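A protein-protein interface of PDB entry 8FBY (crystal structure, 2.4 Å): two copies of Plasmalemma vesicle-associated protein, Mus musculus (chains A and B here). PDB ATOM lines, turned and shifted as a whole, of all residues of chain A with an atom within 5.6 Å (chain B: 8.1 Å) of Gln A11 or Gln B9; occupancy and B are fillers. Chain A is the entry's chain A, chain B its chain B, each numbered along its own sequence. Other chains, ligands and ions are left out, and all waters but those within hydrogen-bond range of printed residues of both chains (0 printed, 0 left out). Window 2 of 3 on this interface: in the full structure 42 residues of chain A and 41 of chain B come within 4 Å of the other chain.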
ATOM      1  N   ARG A   6      17.168 -10.619 -28.406  1.00  0.00           N
ATOM      2  CA  ARG A   6      17.045 -10.352 -29.857  1.00  0.00           C
ATOM      3  C   ARG A   6      15.898  -9.373 -30.119  1.00  0.00           C
ATOM      4  O   ARG A   6      15.903  -8.763 -31.194  1.00  0.00           O
ATOM      5  CB  ARG A   6      16.847 -11.682 -30.586  1.00  0.00           C
ATOM      6  CG  ARG A   6      16.411 -11.541 -32.034  1.00  0.00           C
ATOM      7  CD  ARG A   6      17.498 -11.955 -33.002  1.00  0.00           C
ATOM      8  NE  ARG A   6      16.955 -12.721 -34.114  1.00  0.00           N
ATOM      9  CZ  ARG A   6      16.584 -12.206 -35.279  1.00  0.00           C
ATOM     10  NH1 ARG A   6      16.072 -12.991 -36.212  1.00  0.00           N
ATOM     11  NH2 ARG A   6      16.721 -10.913 -35.504  1.00  0.00           N
ATOM     12  N   GLN A   7      14.985  -9.216 -29.156  1.00  0.00           N
ATOM     13  CA  GLN A   7      13.812  -8.346 -29.299  1.00  0.00           C
ATOM     14  C   GLN A   7      14.141  -6.952 -28.726  1.00  0.00           C
ATOM     15  O   GLN A   7      13.494  -5.966 -29.076  1.00  0.00           O
ATOM     16  CB  GLN A   7      12.548  -8.978 -28.675  1.00  0.00           C
ATOM     17  CG  GLN A   7      12.233  -8.575 -27.233  1.00  0.00           C
ATOM     18  CD  GLN A   7      10.747  -8.580 -26.946  1.00  0.00           C
ATOM     19  OE1 GLN A   7      10.280  -9.213 -25.992  1.00  0.00           O
ATOM     20  NE2 GLN A   7       9.967  -7.868 -27.760  1.00  0.00           N
ATOM     21  N   CYS A   8      15.167  -6.897 -27.852  1.00  0.00           N
ATOM     22  CA  CYS A   8      15.742  -5.695 -27.255  1.00  0.00           C
ATOM     23  C   CYS A   8      16.549  -5.020 -28.361  1.00  0.00           C
ATOM     24  O   CYS A   8      16.429  -3.812 -28.540  1.00  0.00           O
ATOM     25  CB  CYS A   8      16.620  -6.059 -26.058  1.00  0.00           C
ATOM     26  SG  CYS A   8      17.661  -4.706 -25.436  1.00  0.00           S
ATOM     27  N   GLN A   9      17.333  -5.820 -29.127  1.00  0.00           N
ATOM     28  CA  GLN A   9      18.147  -5.375 -30.256  1.00  0.00           C
ATOM     29  C   GLN A   9      17.292  -4.769 -31.373  1.00  0.00           C
ATOM     30  O   GLN A   9      17.642  -3.703 -31.883  1.00  0.00           O
ATOM     31  CB  GLN A   9      19.022  -6.520 -30.796  1.00  0.00           C
ATOM     32  CG  GLN A   9      20.261  -6.799 -29.948  1.00  0.00           C
ATOM     33  CD  GLN A   9      21.327  -5.725 -30.064  1.00  0.00           C
ATOM     34  OE1 GLN A   9      22.170  -5.743 -30.970  1.00  0.00           O
ATOM     35  NE2 GLN A   9      21.317  -4.771 -29.143  1.00  0.00           N
ATOM     36  N   GLU A  10      16.165  -5.440 -31.734  1.00  0.00           N
ATOM     37  CA  GLU A  10      15.220  -4.992 -32.761  1.00  0.00           C
ATOM     38  C   GLU A  10      14.621  -3.634 -32.364  1.00  0.00           C
ATOM     39  O   GLU A  10      14.517  -2.745 -33.213  1.00  0.00           O
ATOM     40  CB  GLU A  10      14.117  -6.050 -32.995  1.00  0.00           C
ATOM     41  CG  GLU A  10      13.157  -5.740 -34.138  1.00  0.00           C
ATOM     42  CD  GLU A  10      13.730  -5.808 -35.542  1.00  0.00           C
ATOM     43  OE1 GLU A  10      14.324  -6.852 -35.900  1.00  0.00           O
ATOM     44  OE2 GLU A  10      13.566  -4.819 -36.295  1.00  0.00           O
ATOM     45  N   GLN A  11      14.283  -3.468 -31.065  1.00  0.00           N
ATOM     46  CA  GLN A  11      13.740  -2.237 -30.496  1.00  0.00           C
ATOM     47  C   GLN A  11      14.749  -1.079 -30.532  1.00  0.00           C
ATOM     48  O   GLN A  11      14.365   0.057 -30.832  1.00  0.00           O
ATOM     49  CB  GLN A  11      13.233  -2.472 -29.068  1.00  0.00           C
ATOM     50  CG  GLN A  11      11.809  -3.024 -29.009  1.00  0.00           C
ATOM     51  CD  GLN A  11      11.161  -2.812 -27.661  1.00  0.00           C
ATOM     52  OE1 GLN A  11      11.723  -3.141 -26.606  1.00  0.00           O
ATOM     53  NE2 GLN A  11       9.950  -2.262 -27.667  1.00  0.00           N
ATOM     54  N   LEU A  12      16.028  -1.359 -30.218  1.00  0.00           N
ATOM     55  CA  LEU A  12      17.098  -0.356 -30.232  1.00  0.00           C
ATOM     56  C   LEU A  12      17.387   0.151 -31.663  1.00  0.00           C
ATOM     57  O   LEU A  12      17.620   1.347 -31.857  1.00  0.00           O
ATOM     58  CB  LEU A  12      18.364  -0.885 -29.538  1.00  0.00           C
ATOM     59  CG  LEU A  12      18.287  -1.014 -28.009  1.00  0.00           C
ATOM     60  CD1 LEU A  12      19.181  -2.098 -27.532  1.00  0.00           C
ATOM     61  CD2 LEU A  12      18.601   0.299 -27.306  1.00  0.00           C
ATOM     62  N   LYS A  13      17.292  -0.752 -32.650  1.00  0.00           N
ATOM     63  CA  LYS A  13      17.430  -0.506 -34.085  1.00  0.00           C
ATOM     64  C   LYS A  13      16.323   0.463 -34.579  1.00  0.00           C
ATOM     65  O   LYS A  13      16.597   1.305 -35.427  1.00  0.00           O
ATOM     66  CB  LYS A  13      17.347  -1.868 -34.846  1.00  0.00           C
ATOM     67  CG  LYS A  13      17.117  -1.791 -36.363  1.00  0.00           C
ATOM     68  CD  LYS A  13      17.381  -3.124 -37.059  1.00  0.00           C
ATOM     69  CE  LYS A  13      16.262  -3.559 -37.985  1.00  0.00           C
ATOM     70  NZ  LYS A  13      16.280  -2.837 -39.292  1.00  0.00           N
ATOM     71  N   GLU A  14      15.094   0.351 -34.019  1.00  0.00           N
ATOM     72  CA  GLU A  14      13.891   1.081 -34.422  1.00  0.00           C
ATOM     73  C   GLU A  14      13.490   2.328 -33.623  1.00  0.00           C
ATOM     74  O   GLU A  14      12.672   3.079 -34.114  1.00  0.00           O
ATOM     75  CB  GLU A  14      12.683   0.101 -34.387  1.00  0.00           C
ATOM     76  CG  GLU A  14      12.728  -1.042 -35.393  1.00  0.00           C
ATOM     77  CD  GLU A  14      12.520  -0.702 -36.860  1.00  0.00           C
ATOM     78  OE1 GLU A  14      11.642   0.138 -37.171  1.00  0.00           O
ATOM     79  OE2 GLU A  14      13.223  -1.303 -37.706  1.00  0.00           O
ATOM     80  N   VAL A  15      13.950   2.496 -32.381  1.00  0.00           N
ATOM     81  CA  VAL A  15      13.461   3.537 -31.455  1.00  0.00           C
ATOM     82  C   VAL A  15      13.553   4.997 -32.009  1.00  0.00           C
ATOM     83  O   VAL A  15      12.582   5.737 -31.881  1.00  0.00           O
ATOM     84  CB  VAL A  15      14.089   3.406 -30.035  1.00  0.00           C
ATOM     85  CG1 VAL A  15      15.618   3.533 -30.040  1.00  0.00           C
ATOM     86  CG2 VAL A  15      13.454   4.366 -29.039  1.00  0.00           C
ATOM     87  N   SER B   5      14.858  -6.858 -21.744  1.00  0.00           N
ATOM     88  CA  SER B   5      13.762  -5.964 -21.370  1.00  0.00           C
ATOM     89  C   SER B   5      13.921  -5.389 -19.942  1.00  0.00           C
ATOM     90  O   SER B   5      12.984  -4.781 -19.418  1.00  0.00           O
ATOM     91  CB  SER B   5      12.418  -6.674 -21.537  1.00  0.00           C
ATOM     92  OG  SER B   5      11.327  -5.787 -21.347  1.00  0.00           O
ATOM     93  N   ARG B   6      15.116  -5.550 -19.336  1.00  0.00           N
ATOM     94  CA  ARG B   6      15.418  -5.082 -17.976  1.00  0.00           C
ATOM     95  C   ARG B   6      15.993  -3.643 -17.980  1.00  0.00           C
ATOM     96  O   ARG B   6      15.260  -2.680 -17.730  1.00  0.00           O
ATOM     97  CB  ARG B   6      16.367  -6.085 -17.276  1.00  0.00           C
ATOM     98  CG  ARG B   6      16.412  -5.968 -15.756  1.00  0.00           C
ATOM     99  CD  ARG B   6      17.749  -6.431 -15.207  1.00  0.00           C
ATOM    100  NE  ARG B   6      18.796  -5.417 -15.370  1.00  0.00           N
ATOM    101  CZ  ARG B   6      19.292  -4.676 -14.383  1.00  0.00           C
ATOM    102  NH1 ARG B   6      18.859  -4.836 -13.138  1.00  0.00           N
ATOM    103  NH2 ARG B   6      20.235  -3.777 -14.631  1.00  0.00           N
ATOM    104  N   GLN B   7      17.306  -3.513 -18.258  1.00  0.00           N
ATOM    105  CA  GLN B   7      18.002  -2.228 -18.364  1.00  0.00           C
ATOM    106  C   GLN B   7      17.881  -1.717 -19.814  1.00  0.00           C
ATOM    107  O   GLN B   7      18.328  -0.611 -20.117  1.00  0.00           O
ATOM    108  CB  GLN B   7      19.482  -2.323 -17.890  1.00  0.00           C
ATOM    109  CG  GLN B   7      20.355  -3.399 -18.566  1.00  0.00           C
ATOM    110  CD  GLN B   7      20.731  -3.095 -20.011  1.00  0.00           C
ATOM    111  OE1 GLN B   7      20.153  -3.652 -20.951  1.00  0.00           O
ATOM    112  NE2 GLN B   7      21.700  -2.206 -20.226  1.00  0.00           N
ATOM    113  N   CYS B   8      17.296  -2.559 -20.699  1.00  0.00           N
ATOM    114  CA  CYS B   8      17.056  -2.298 -22.117  1.00  0.00           C
ATOM    115  C   CYS B   8      16.047  -1.182 -22.264  1.00  0.00           C
ATOM    116  O   CYS B   8      16.246  -0.296 -23.091  1.00  0.00           O
ATOM    117  CB  CYS B   8      16.590  -3.564 -22.831  1.00  0.00           C
ATOM    118  SG  CYS B   8      16.352  -3.370 -24.621  1.00  0.00           S
ATOM    119  N   GLN B   9      14.977  -1.211 -21.442  1.00  0.00           N
ATOM    120  CA  GLN B   9      13.941  -0.176 -21.460  1.00  0.00           C
ATOM    121  C   GLN B   9      14.469   1.185 -20.989  1.00  0.00           C
ATOM    122  O   GLN B   9      14.057   2.208 -21.531  1.00  0.00           O
ATOM    123  CB  GLN B   9      12.683  -0.611 -20.702  1.00  0.00           C
ATOM    124  CG  GLN B   9      11.702  -1.397 -21.586  1.00  0.00           C
ATOM    125  CD  GLN B   9      11.095  -0.608 -22.744  1.00  0.00           C
ATOM    126  OE1 GLN B   9      11.017   0.636 -22.742  1.00  0.00           O
ATOM    127  NE2 GLN B   9      10.631  -1.328 -23.762  1.00  0.00           N
ATOM    128  N   GLU B  10      15.437   1.187 -20.053  1.00  0.00           N
ATOM    129  CA  GLU B  10      16.104   2.395 -19.567  1.00  0.00           C
ATOM    130  C   GLU B  10      17.073   2.917 -20.637  1.00  0.00           C
ATOM    131  O   GLU B  10      17.357   4.116 -20.680  1.00  0.00           O
ATOM    132  CB  GLU B  10      16.835   2.126 -18.242  1.00  0.00           C
ATOM    133  CG  GLU B  10      16.673   3.229 -17.203  1.00  0.00           C
ATOM    134  CD  GLU B  10      15.255   3.546 -16.753  1.00  0.00           C
ATOM    135  OE1 GLU B  10      14.464   2.599 -16.533  1.00  0.00           O
ATOM    136  OE2 GLU B  10      14.938   4.749 -16.615  1.00  0.00           O
ATOM    137  N   GLN B  11      17.555   2.012 -21.514  1.00  0.00           N
ATOM    138  CA  GLN B  11      18.434   2.358 -22.627  1.00  0.00           C
ATOM    139  C   GLN B  11      17.613   3.014 -23.751  1.00  0.00           C
ATOM    140  O   GLN B  11      18.015   4.057 -24.263  1.00  0.00           O
ATOM    141  CB  GLN B  11      19.196   1.127 -23.151  1.00  0.00           C
ATOM    142  CG  GLN B  11      20.371   1.496 -24.048  1.00  0.00           C
ATOM    143  CD  GLN B  11      21.576   1.937 -23.256  1.00  0.00           C
ATOM    144  OE1 GLN B  11      22.416   1.118 -22.873  1.00  0.00           O
ATOM    145  NE2 GLN B  11      21.688   3.238 -22.994  1.00  0.00           N
ATOM    146  N   LEU B  12      16.464   2.410 -24.103  1.00  0.00           N
ATOM    147  CA  LEU B  12      15.533   2.888 -25.123  1.00  0.00           C
ATOM    148  C   LEU B  12      15.005   4.295 -24.787  1.00  0.00           C
ATOM    149  O   LEU B  12      14.835   5.130 -25.680  1.00  0.00           O
ATOM    150  CB  LEU B  12      14.368   1.889 -25.282  1.00  0.00           C
ATOM    151  CG  LEU B  12      14.703   0.581 -26.017  1.00  0.00           C
ATOM    152  CD1 LEU B  12      13.796  -0.540 -25.573  1.00  0.00           C
ATOM    153  CD2 LEU B  12      14.667   0.754 -27.533  1.00  0.00           C
ATOM    154  N   LYS B  13      14.792   4.543 -23.485  1.00  0.00           N
ATOM    155  CA  LYS B  13      14.333   5.793 -22.922  1.00  0.00           C
ATOM    156  C   LYS B  13      15.373   6.889 -23.082  1.00  0.00           C
ATOM    157  O   LYS B  13      15.033   7.953 -23.606  1.00  0.00           O
ATOM    158  CB  LYS B  13      13.931   5.614 -21.443  1.00  0.00           C
ATOM    159  CG  LYS B  13      12.423   5.413 -21.257  1.00  0.00           C
ATOM    160  CD  LYS B  13      12.042   4.343 -20.216  1.00  0.00           C
ATOM    161  CE  LYS B  13      11.956   4.823 -18.786  1.00  0.00           C
ATOM    162  NZ  LYS B  13      11.284   3.815 -17.918  1.00  0.00           N
ATOM    163  N   GLU B  14      16.627   6.650 -22.651  1.00  0.00           N
ATOM    164  CA  GLU B  14      17.663   7.679 -22.743  1.00  0.00           C
ATOM    165  C   GLU B  14      18.094   8.025 -24.184  1.00  0.00           C
ATOM    166  O   GLU B  14      18.403   9.194 -24.437  1.00  0.00           O
ATOM    167  CB  GLU B  14      18.884   7.366 -21.870  1.00  0.00           C
ATOM    168  CG  GLU B  14      18.891   8.136 -20.545  1.00  0.00           C
ATOM    169  CD  GLU B  14      18.831   9.662 -20.568  1.00  0.00           C
ATOM    170  OE1 GLU B  14      19.417  10.278 -21.492  1.00  0.00           O
ATOM    171  OE2 GLU B  14      18.207  10.243 -19.646  1.00  0.00           O
ATOM    172  N   VAL B  15      18.098   7.042 -25.113  1.00  0.00           N
ATOM    173  CA  VAL B  15      18.501   7.303 -26.491  1.00  0.00           C
ATOM    174  C   VAL B  15      17.435   8.174 -27.201  1.00  0.00           C
ATOM    175  O   VAL B  15      17.794   9.144 -27.858  1.00  0.00           O
ATOM    176  CB  VAL B  15      18.942   6.039 -27.317  1.00  0.00           C
ATOM    177  CG1 VAL B  15      20.118   5.331 -26.656  1.00  0.00           C
ATOM    178  CG2 VAL B  15      17.804   5.065 -27.560  1.00  0.00           C
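SG of Cys A8 forms a disulfide with SG of Cys B8, at 2.0 Å.
Gln B9 touches Gln A11 (NE2 to OE1, 3.5 Å).
Gln A11 touches Leu B12.
CD2 of Leu A12 touches CG of Gln B11, 3.9 Å away.
Leu A12 touches Leu B12 (N to CD2, 3.7 Å).
Val A15 touches Leu B12 (CB to CD2, 3.7 Å).
Val B15 touches Val A15.
Gln A11 touches just these residues of chain B: Gln B9 (3.5 Å) and Leu B12 (3.4 Å).
Printed residues of chain B within 4 Å of Val A15: Leu B12 and Val B15.
Printed residues of chain A within 4 Å of Cys B8: Cys A8.
Gln B9 touches just one residue of chain A: Gln A11.
Of the printed residues of chain A, Gln B11 touches Leu A12.
Of the printed residues of chain A, Leu B12 touches Gln A11, Leu A12 and Val A15.
Printed residues of chain A within 4 Å of Val B15: Val A15.
The nearest residue of chain B that does not touch Gln A11 is Cys B8 (5.0 Å).
The nearest printed residue of chain A that does not touch Gln B9 is Cys A8 (5.9 Å).
The nearest printed residue of chain A that does not touch Leu B12 is Cys A8 (5.0 Å).
Hydrophobic or aromatic side chains of chain A that line the printed part of chain B: Leu A12 and Val A15.
Hydrophobic or aromatic side chains of chain B within 4 Å of the printed part of chain A: Leu B12 and Val B15.
Among the printed residues, 7 pairs touch across the chains.
Among the printed residues, no Asp or Glu carboxylate lies within 4 Å of a Lys or Arg side-chain nitrogen of the other chain.
Cys B8 touches its own counterpart, Cys A8.
Gln A11 touches Gln B9, but with the chains exchanged Gln A9 does not touch Gln B11 (8.1 Å).
Leu A12 touches its own counterpart, Leu B12.
Val A15 touches its own counterpart, Val B15.
Positions printed for both chains: 6, 7, 8, 9, 10, 11, 12, 13, 14 and 15.
Of the 7 pairs that touch across the chains among the printed residues, 5 have their exchanged pair printed and touching as well.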
